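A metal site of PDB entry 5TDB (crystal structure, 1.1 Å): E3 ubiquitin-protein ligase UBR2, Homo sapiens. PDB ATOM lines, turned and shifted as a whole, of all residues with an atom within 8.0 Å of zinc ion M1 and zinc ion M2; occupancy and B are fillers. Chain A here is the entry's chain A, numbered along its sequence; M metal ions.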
ATOM      1  N   LEU A   6     -19.959 -32.451  21.341  1.00  0.00           N
ATOM      2  CA  LEU A   6     -18.698 -31.758  21.048  1.00  0.00           C
ATOM      3  C   LEU A   6     -18.885 -30.262  20.757  1.00  0.00           C
ATOM      4  O   LEU A   6     -17.893 -29.556  20.492  1.00  0.00           O
ATOM      5  CB  LEU A   6     -17.963 -32.458  19.891  1.00  0.00           C
ATOM      6  N   CYS A   7     -20.129 -29.774  20.770  1.00  0.00           N
ATOM      7  CA  CYS A   7     -20.376 -28.333  20.724  1.00  0.00           C
ATOM      8  C   CYS A   7     -20.006 -27.698  22.060  1.00  0.00           C
ATOM      9  O   CYS A   7     -19.005 -26.985  22.149  1.00  0.00           O
ATOM     10  CB  CYS A   7     -21.834 -28.032  20.376  1.00  0.00           C
ATOM     11  SG  CYS A   7     -22.080 -26.261  20.333  1.00  0.00           S
ATOM     12  N   GLY A   8     -20.805 -27.951  23.096  1.00  0.00           N
ATOM     13  CA  GLY A   8     -20.568 -27.406  24.425  1.00  0.00           C
ATOM     14  C   GLY A   8     -20.704 -25.897  24.560  1.00  0.00           C
ATOM     15  O   GLY A   8     -20.369 -25.377  25.630  1.00  0.00           O
ATOM     16  N   ARG A   9     -21.208 -25.193  23.546  1.00  0.00           N
ATOM     17  CA  ARG A   9     -21.211 -23.728  23.564  1.00  0.00           C
ATOM     18  C   ARG A   9     -21.891 -23.198  24.812  1.00  0.00           C
ATOM     19  O   ARG A   9     -23.016 -23.576  25.124  1.00  0.00           O
ATOM     20  CB  ARG A   9     -21.955 -23.187  22.335  1.00  0.00           C
ATOM     21  CG  ARG A   9     -21.954 -21.644  22.259  1.00  0.00           C
ATOM     22  CD  ARG A   9     -22.951 -21.034  21.272  1.00  0.00           C
ATOM     23  NE  ARG A   9     -22.688 -21.424  19.897  1.00  0.00           N
ATOM     24  CZ  ARG A   9     -22.999 -20.689  18.824  1.00  0.00           C
ATOM     25  NH1 ARG A   9     -23.554 -19.486  18.943  1.00  0.00           N
ATOM     26  NH2 ARG A   9     -22.718 -21.136  17.616  1.00  0.00           N
ATOM     27  N   VAL A  10     -21.222 -22.272  25.511  1.00  0.00           N
ATOM     28  CA  VAL A  10     -21.810 -21.558  26.640  1.00  0.00           C
ATOM     29  C   VAL A  10     -22.463 -20.284  26.116  1.00  0.00           C
ATOM     30  O   VAL A  10     -21.832 -19.496  25.398  1.00  0.00           O
ATOM     31  CB  VAL A  10     -20.747 -21.244  27.701  1.00  0.00           C
ATOM     32  CG1 VAL A  10     -21.350 -20.371  28.798  1.00  0.00           C
ATOM     33  CG2 VAL A  10     -20.207 -22.528  28.274  1.00  0.00           C
ATOM     34  N   PHE A  11     -23.737 -20.098  26.439  1.00  0.00           N
ATOM     35  CA  PHE A  11     -24.493 -18.964  25.906  1.00  0.00           C
ATOM     36  C   PHE A  11     -24.061 -17.642  26.520  1.00  0.00           C
ATOM     37  O   PHE A  11     -23.767 -17.540  27.718  1.00  0.00           O
ATOM     38  CB  PHE A  11     -25.993 -19.163  26.099  1.00  0.00           C
ATOM     39  CG  PHE A  11     -26.507 -20.376  25.415  1.00  0.00           C
ATOM     40  CD1 PHE A  11     -26.446 -20.484  24.042  1.00  0.00           C
ATOM     41  CD2 PHE A  11     -27.024 -21.437  26.153  1.00  0.00           C
ATOM     42  CE1 PHE A  11     -26.912 -21.602  23.406  1.00  0.00           C
ATOM     43  CE2 PHE A  11     -27.491 -22.563  25.512  1.00  0.00           C
ATOM     44  CZ  PHE A  11     -27.418 -22.655  24.148  1.00  0.00           C
ATOM     45  N   GLU A  15     -28.205 -14.094  23.855  1.00  0.00           N
ATOM     46  CA  GLU A  15     -28.051 -15.024  22.741  1.00  0.00           C
ATOM     47  C   GLU A  15     -29.282 -15.928  22.614  1.00  0.00           C
ATOM     48  O   GLU A  15     -29.762 -16.471  23.622  1.00  0.00           O
ATOM     49  CB  GLU A  15     -26.811 -15.862  22.947  1.00  0.00           C
ATOM     50  CG  GLU A  15     -26.430 -16.630  21.738  1.00  0.00           C
ATOM     51  CD  GLU A  15     -25.127 -17.396  21.899  1.00  0.00           C
ATOM     52  OE1 GLU A  15     -24.946 -18.334  21.124  1.00  0.00           O
ATOM     53  OE2 GLU A  15     -24.289 -17.104  22.769  1.00  0.00           O
ATOM     54  N   VAL A  30     -31.686 -27.563  25.198  1.00  0.00           N
ATOM     55  CA  VAL A  30     -31.586 -26.496  24.211  1.00  0.00           C
ATOM     56  C   VAL A  30     -30.430 -26.751  23.257  1.00  0.00           C
ATOM     57  O   VAL A  30     -29.481 -27.477  23.544  1.00  0.00           O
ATOM     58  CB  VAL A  30     -31.429 -25.115  24.876  1.00  0.00           C
ATOM     59  CG1 VAL A  30     -32.705 -24.721  25.601  1.00  0.00           C
ATOM     60  CG2 VAL A  30     -30.227 -25.120  25.807  1.00  0.00           C
ATOM     61  N   LEU A  31     -30.531 -26.088  22.110  1.00  0.00           N
ATOM     62  CA  LEU A  31     -29.495 -26.019  21.101  1.00  0.00           C
ATOM     63  C   LEU A  31     -29.101 -24.570  20.828  1.00  0.00           C
ATOM     64  O   LEU A  31     -29.946 -23.662  20.856  1.00  0.00           O
ATOM     65  CB  LEU A  31     -29.972 -26.645  19.789  1.00  0.00           C
ATOM     66  CG  LEU A  31     -30.298 -28.138  19.868  1.00  0.00           C
ATOM     67  CD1 LEU A  31     -30.885 -28.609  18.564  1.00  0.00           C
ATOM     68  CD2 LEU A  31     -29.084 -28.968  20.222  1.00  0.00           C
ATOM     69  N   CYS A  32     -27.807 -24.366  20.560  1.00  0.00           N
ATOM     70  CA  CYS A  32     -27.340 -23.074  20.061  1.00  0.00           C
ATOM     71  C   CYS A  32     -27.826 -22.876  18.628  1.00  0.00           C
ATOM     72  O   CYS A  32     -28.325 -23.790  17.971  1.00  0.00           O
ATOM     73  CB  CYS A  32     -25.814 -22.965  20.148  1.00  0.00           C
ATOM     74  SG  CYS A  32     -24.899 -23.967  18.917  1.00  0.00           S
ATOM     75  N   MET A  33     -27.643 -21.662  18.132  1.00  0.00           N
ATOM     76  CA  MET A  33     -28.131 -21.339  16.802  1.00  0.00           C
ATOM     77  C   MET A  33     -27.502 -22.227  15.739  1.00  0.00           C
ATOM     78  O   MET A  33     -28.178 -22.682  14.810  1.00  0.00           O
ATOM     79  CB  MET A  33     -27.838 -19.864  16.528  1.00  0.00           C
ATOM     80  CG  MET A  33     -28.304 -19.389  15.205  1.00  0.00           C
ATOM     81  SD  MET A  33     -27.750 -17.702  14.916  1.00  0.00           S
ATOM     82  CE  MET A  33     -27.789 -17.778  13.133  1.00  0.00           C
ATOM     83  N   GLU A  34     -26.179 -22.438  15.826  1.00  0.00           N
ATOM     84  CA  GLU A  34     -25.500 -23.251  14.821  1.00  0.00           C
ATOM     85  C   GLU A  34     -26.067 -24.661  14.789  1.00  0.00           C
ATOM     86  O   GLU A  34     -26.361 -25.222  13.719  1.00  0.00           O
ATOM     87  CB  GLU A  34     -23.998 -23.293  15.126  1.00  0.00           C
ATOM     88  CG  GLU A  34     -23.248 -24.231  14.181  1.00  0.00           C
ATOM     89  CD  GLU A  34     -21.778 -24.412  14.478  1.00  0.00           C
ATOM     90  OE1 GLU A  34     -21.313 -23.926  15.539  1.00  0.00           O
ATOM     91  OE2 GLU A  34     -21.108 -25.067  13.652  1.00  0.00           O
ATOM     92  N   CYS A  35     -26.215 -25.262  15.962  1.00  0.00           N
ATOM     93  CA  CYS A  35     -26.671 -26.643  16.044  1.00  0.00           C
ATOM     94  C   CYS A  35     -28.138 -26.765  15.652  1.00  0.00           C
ATOM     95  O   CYS A  35     -28.509 -27.683  14.909  1.00  0.00           O
ATOM     96  CB  CYS A  35     -26.375 -27.189  17.445  1.00  0.00           C
ATOM     97  SG  CYS A  35     -24.592 -27.291  17.733  1.00  0.00           S
ATOM     98  N   PHE A  36     -28.973 -25.818  16.094  1.00  0.00           N
ATOM     99  CA  PHE A  36     -30.384 -25.827  15.725  1.00  0.00           C
ATOM    100  C   PHE A  36     -30.551 -25.814  14.202  1.00  0.00           C
ATOM    101  O   PHE A  36     -31.316 -26.610  13.651  1.00  0.00           O
ATOM    102  CB  PHE A  36     -31.103 -24.621  16.372  1.00  0.00           C
ATOM    103  CG  PHE A  36     -32.487 -24.423  15.862  1.00  0.00           C
ATOM    104  CD1 PHE A  36     -33.516 -25.295  16.211  1.00  0.00           C
ATOM    105  CD2 PHE A  36     -32.789 -23.349  15.021  1.00  0.00           C
ATOM    106  CE1 PHE A  36     -34.804 -25.090  15.727  1.00  0.00           C
ATOM    107  CE2 PHE A  36     -34.056 -23.165  14.544  1.00  0.00           C
ATOM    108  CZ  PHE A  36     -35.053 -24.042  14.896  1.00  0.00           C
ATOM    109  N   GLY A  38     -28.636 -26.726  11.871  1.00  0.00           N
ATOM    110  CA  GLY A  38     -28.136 -27.933  11.246  1.00  0.00           C
ATOM    111  C   GLY A  38     -28.760 -29.217  11.777  1.00  0.00           C
ATOM    112  O   GLY A  38     -28.215 -30.310  11.540  1.00  0.00           O
ATOM    113  N   SER A  39     -29.914 -29.107  12.449  1.00  0.00           N
ATOM    114  CA  SER A  39     -30.554 -30.240  13.118  1.00  0.00           C
ATOM    115  C   SER A  39     -31.911 -30.529  12.473  1.00  0.00           C
ATOM    116  O   SER A  39     -32.470 -29.717  11.735  1.00  0.00           O
ATOM    117  CB  SER A  39     -30.777 -29.952  14.612  1.00  0.00           C
ATOM    118  OG  SER A  39     -31.893 -29.098  14.833  1.00  0.00           O
ATOM    119  N   PHE A  56     -25.693 -23.962  28.486  1.00  0.00           N
ATOM    120  CA  PHE A  56     -24.872 -24.511  27.413  1.00  0.00           C
ATOM    121  C   PHE A  56     -25.730 -25.315  26.435  1.00  0.00           C
ATOM    122  O   PHE A  56     -26.812 -25.819  26.761  1.00  0.00           O
ATOM    123  CB  PHE A  56     -23.689 -25.341  27.947  1.00  0.00           C
ATOM    124  CG  PHE A  56     -24.107 -26.525  28.790  1.00  0.00           C
ATOM    125  CD1 PHE A  56     -24.393 -27.746  28.199  1.00  0.00           C
ATOM    126  CD2 PHE A  56     -24.228 -26.404  30.171  1.00  0.00           C
ATOM    127  CE1 PHE A  56     -24.805 -28.823  28.958  1.00  0.00           C
ATOM    128  CE2 PHE A  56     -24.618 -27.478  30.940  1.00  0.00           C
ATOM    129  CZ  PHE A  56     -24.906 -28.687  30.333  1.00  0.00           C
ATOM    130  N   CYS A  57     -25.183 -25.482  25.236  1.00  0.00           N
ATOM    131  CA  CYS A  57     -25.830 -26.243  24.180  1.00  0.00           C
ATOM    132  C   CYS A  57     -25.774 -27.741  24.478  1.00  0.00           C
ATOM    133  O   CYS A  57     -24.726 -28.254  24.866  1.00  0.00           O
ATOM    134  CB  CYS A  57     -25.108 -25.945  22.866  1.00  0.00           C
ATOM    135  SG  CYS A  57     -25.758 -26.852  21.441  1.00  0.00           S
ATOM    136  N   ASP A  58     -26.899 -28.429  24.254  1.00  0.00           N
ATOM    137  CA  ASP A  58     -27.043 -29.854  24.502  1.00  0.00           C
ATOM    138  C   ASP A  58     -26.883 -30.707  23.243  1.00  0.00           C
ATOM    139  O   ASP A  58     -27.250 -31.890  23.256  1.00  0.00           O
ATOM    140  CB  ASP A  58     -28.382 -30.145  25.163  1.00  0.00           C
ATOM    141  CG  ASP A  58     -28.520 -29.473  26.499  1.00  0.00           C
ATOM    142  OD1 ASP A  58     -27.640 -29.687  27.381  1.00  0.00           O
ATOM    143  OD2 ASP A  58     -29.490 -28.699  26.687  1.00  0.00           O
ATOM    144  N   CYS A  59     -26.335 -30.146  22.162  1.00  0.00           N
ATOM    145  CA  CYS A  59     -26.081 -30.941  20.980  1.00  0.00           C
ATOM    146  C   CYS A  59     -25.152 -32.093  21.334  1.00  0.00           C
ATOM    147  O   CYS A  59     -24.086 -31.897  21.935  1.00  0.00           O
ATOM    148  CB  CYS A  59     -25.431 -30.078  19.889  1.00  0.00           C
ATOM    149  SG  CYS A  59     -24.961 -31.049  18.431  1.00  0.00           S
ATOM    150  N   GLY A  60     -25.556 -33.292  20.942  1.00  0.00           N
ATOM    151  CA  GLY A  60     -24.789 -34.475  21.176  1.00  0.00           C
ATOM    152  C   GLY A  60     -25.136 -35.224  22.436  1.00  0.00           C
ATOM    153  O   GLY A  60     -24.606 -36.324  22.646  1.00  0.00           O
ATOM    154  N   PRO A  69     -30.359 -36.150  18.382  1.00  0.00           N
ATOM    155  CA  PRO A  69     -29.496 -35.492  19.390  1.00  0.00           C
ATOM    156  C   PRO A  69     -28.344 -34.697  18.815  1.00  0.00           C
ATOM    157  O   PRO A  69     -27.864 -33.774  19.481  1.00  0.00           O
ATOM    158  CB  PRO A  69     -29.009 -36.665  20.252  1.00  0.00           C
ATOM    159  CG  PRO A  69     -29.064 -37.825  19.343  1.00  0.00           C
ATOM    160  CD  PRO A  69     -30.284 -37.622  18.485  1.00  0.00           C
ATOM    161  N   TYR A  70     -27.868 -35.030  17.619  1.00  0.00           N
ATOM    162  CA  TYR A  70     -26.730 -34.340  17.020  1.00  0.00           C
ATOM    163  C   TYR A  70     -27.197 -33.538  15.810  1.00  0.00           C
ATOM    164  O   TYR A  70     -28.117 -33.940  15.110  1.00  0.00           O
ATOM    165  CB  TYR A  70     -25.676 -35.357  16.553  1.00  0.00           C
ATOM    166  CG  TYR A  70     -24.843 -36.025  17.650  1.00  0.00           C
ATOM    167  CD1 TYR A  70     -25.249 -37.196  18.264  1.00  0.00           C
ATOM    168  CD2 TYR A  70     -23.628 -35.471  18.049  1.00  0.00           C
ATOM    169  CE1 TYR A  70     -24.476 -37.813  19.246  1.00  0.00           C
ATOM    170  CE2 TYR A  70     -22.844 -36.080  19.035  1.00  0.00           C
ATOM    171  CZ  TYR A  70     -23.283 -37.239  19.638  1.00  0.00           C
ATOM    172  OH  TYR A  70     -22.500 -37.842  20.616  1.00  0.00           O
ATOM    173  N   CYS A  71     -26.527 -32.417  15.552  1.00  0.00           N
ATOM    174  CA  CYS A  71     -26.646 -31.677  14.301  1.00  0.00           C
ATOM    175  C   CYS A  71     -25.658 -32.217  13.256  1.00  0.00           C
ATOM    176  O   CYS A  71     -24.810 -33.052  13.543  1.00  0.00           O
ATOM    177  CB  CYS A  71     -26.394 -30.195  14.563  1.00  0.00           C
ATOM    178  SG  CYS A  71     -24.655 -29.739  14.766  1.00  0.00           S
ATOM    179  N   GLN A  72     -25.762 -31.695  12.031  1.00  0.00           N
ATOM    180  CA  GLN A  72     -24.912 -32.180  10.950  1.00  0.00           C
ATOM    181  C   GLN A  72     -23.432 -31.870  11.178  1.00  0.00           C
ATOM    182  O   GLN A  72     -22.568 -32.584  10.663  1.00  0.00           O
ATOM    183  CB  GLN A  72     -25.326 -31.544   9.635  1.00  0.00           C
ATOM    184  CG  GLN A  72     -26.654 -31.979   9.104  1.00  0.00           C
ATOM    185  CD  GLN A  72     -26.892 -31.491   7.689  1.00  0.00           C
ATOM    186  OE1 GLN A  72     -26.963 -30.281   7.434  1.00  0.00           O
ATOM    187  NE2 GLN A  72     -26.993 -32.414   6.749  1.00  0.00           N
ATOM    188  N   LYS A  73     -23.122 -30.817  11.916  1.00  0.00           N
ATOM    189  CA  LYS A  73     -21.741 -30.443  12.157  1.00  0.00           C
ATOM    190  C   LYS A  73     -21.070 -31.324  13.200  1.00  0.00           C
ATOM    191  O   LYS A  73     -19.848 -31.537  13.116  1.00  0.00           O
ATOM    192  CB  LYS A  73     -21.705 -28.967  12.587  1.00  0.00           C
ATOM    193  CG  LYS A  73     -20.356 -28.289  12.456  1.00  0.00           C
ATOM    194  CD  LYS A  73     -19.722 -28.125  13.804  1.00  0.00           C
ATOM    195  CE  LYS A  73     -18.406 -27.348  13.712  1.00  0.00           C
ATOM    196  NZ  LYS A  73     -18.573 -25.894  13.425  1.00  0.00           N
ATOM    197  N   HIS A  74     -21.820 -31.858  14.173  1.00  0.00           N
ATOM    198  CA  HIS A  74     -21.209 -32.588  15.274  1.00  0.00           C
ATOM    199  C   HIS A  74     -21.454 -34.091  15.232  1.00  0.00           C
ATOM    200  O   HIS A  74     -20.776 -34.832  15.953  1.00  0.00           O
ATOM    201  CB  HIS A  74     -21.668 -31.999  16.628  1.00  0.00           C
ATOM    202  CG  HIS A  74     -21.192 -30.598  16.843  1.00  0.00           C
ATOM    203  ND1 HIS A  74     -22.040 -29.505  16.906  1.00  0.00           N
ATOM    204  CD2 HIS A  74     -19.935 -30.112  16.949  1.00  0.00           C
ATOM    205  CE1 HIS A  74     -21.306 -28.414  17.028  1.00  0.00           C
ATOM    206  NE2 HIS A  74     -20.031 -28.753  17.079  1.00  0.00           N
ATOM    207  N   GLU A  75     -22.343 -34.571  14.359  1.00  0.00           N
ATOM    208  CA  GLU A  75     -22.608 -36.006  14.258  1.00  0.00           C
ATOM    209  C   GLU A  75     -21.379 -36.781  13.801  1.00  0.00           C
ATOM    210  O   GLU A  75     -21.291 -37.977  14.102  1.00  0.00           O
ATOM    211  CB  GLU A  75     -23.743 -36.263  13.251  1.00  0.00           C
ATOM    212  CG  GLU A  75     -23.379 -35.959  11.801  1.00  0.00           C
ATOM    213  CD  GLU A  75     -24.526 -36.173  10.839  1.00  0.00           C
ATOM    214  OE1 GLU A  75     -25.434 -36.957  11.182  1.00  0.00           O
ATOM    215  OE2 GLU A  75     -24.518 -35.556   9.739  1.00  0.00           O
HETATM  216 ZN    ZN M   1     -24.112 -29.483  17.007  1.00  0.00          ZN
HETATM  217 ZN    ZN M   2     -24.324 -26.071  19.774  1.00  0.00          ZN
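Zinc ion M2 is bound by the side-chain sulfur (SG) of Cys 7, at 2.3 Å.
SG of Cys 57 is bound to zinc ion M2, 2.3 Å away.
SG of Cys 32 binds zinc ion M2, at 2.3 Å.
Zinc ion M2 is bound by SG of Cys 35.
Zinc ion M2 has four donor atoms within binding distance.
Zinc ion M1 is bound by a ring nitrogen (ND1) of His 74 (2.1 Å), the side-chain sulfur (SG) of Cys 59 (2.3 Å), the side-chain sulfur (SG) of Cys 71 (2.3 Å) and the side-chain sulfur (SG) of Cys 35 (2.4 Å).
Zinc ion M1 has four donor atoms within binding distance.
Four residues have an atom within 4 Å of zinc ion M1: Cys 35, Cys 59, Cys 71 and His 74.
The nearest printed residue that does not touch zinc ion M1 is Cys 7 (4.3 Å).
The backbone NH of Cys 59 lies close to the side-chain sulfur of Cys 57.
The side-chain sulfur (SG) of Cys 7 sits close to the backbone NH (N) of Arg 9 (3.5 Å).
SG of Cys 71 sits close to N of Lys 73 (3.4 Å).
The backbone NH of Cys 57 sits at hydrogen-bond distance from the backbone carbonyl oxygen of Arg 9, 2.9 Å away.
The guanidinium group of Arg 9 sits close to the side-chain sulfur of Cys 32, 3.5 Å away.
The side-chain sulfur of Cys 32 lies close to the backbone NH of Glu 34 (3.7 Å).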
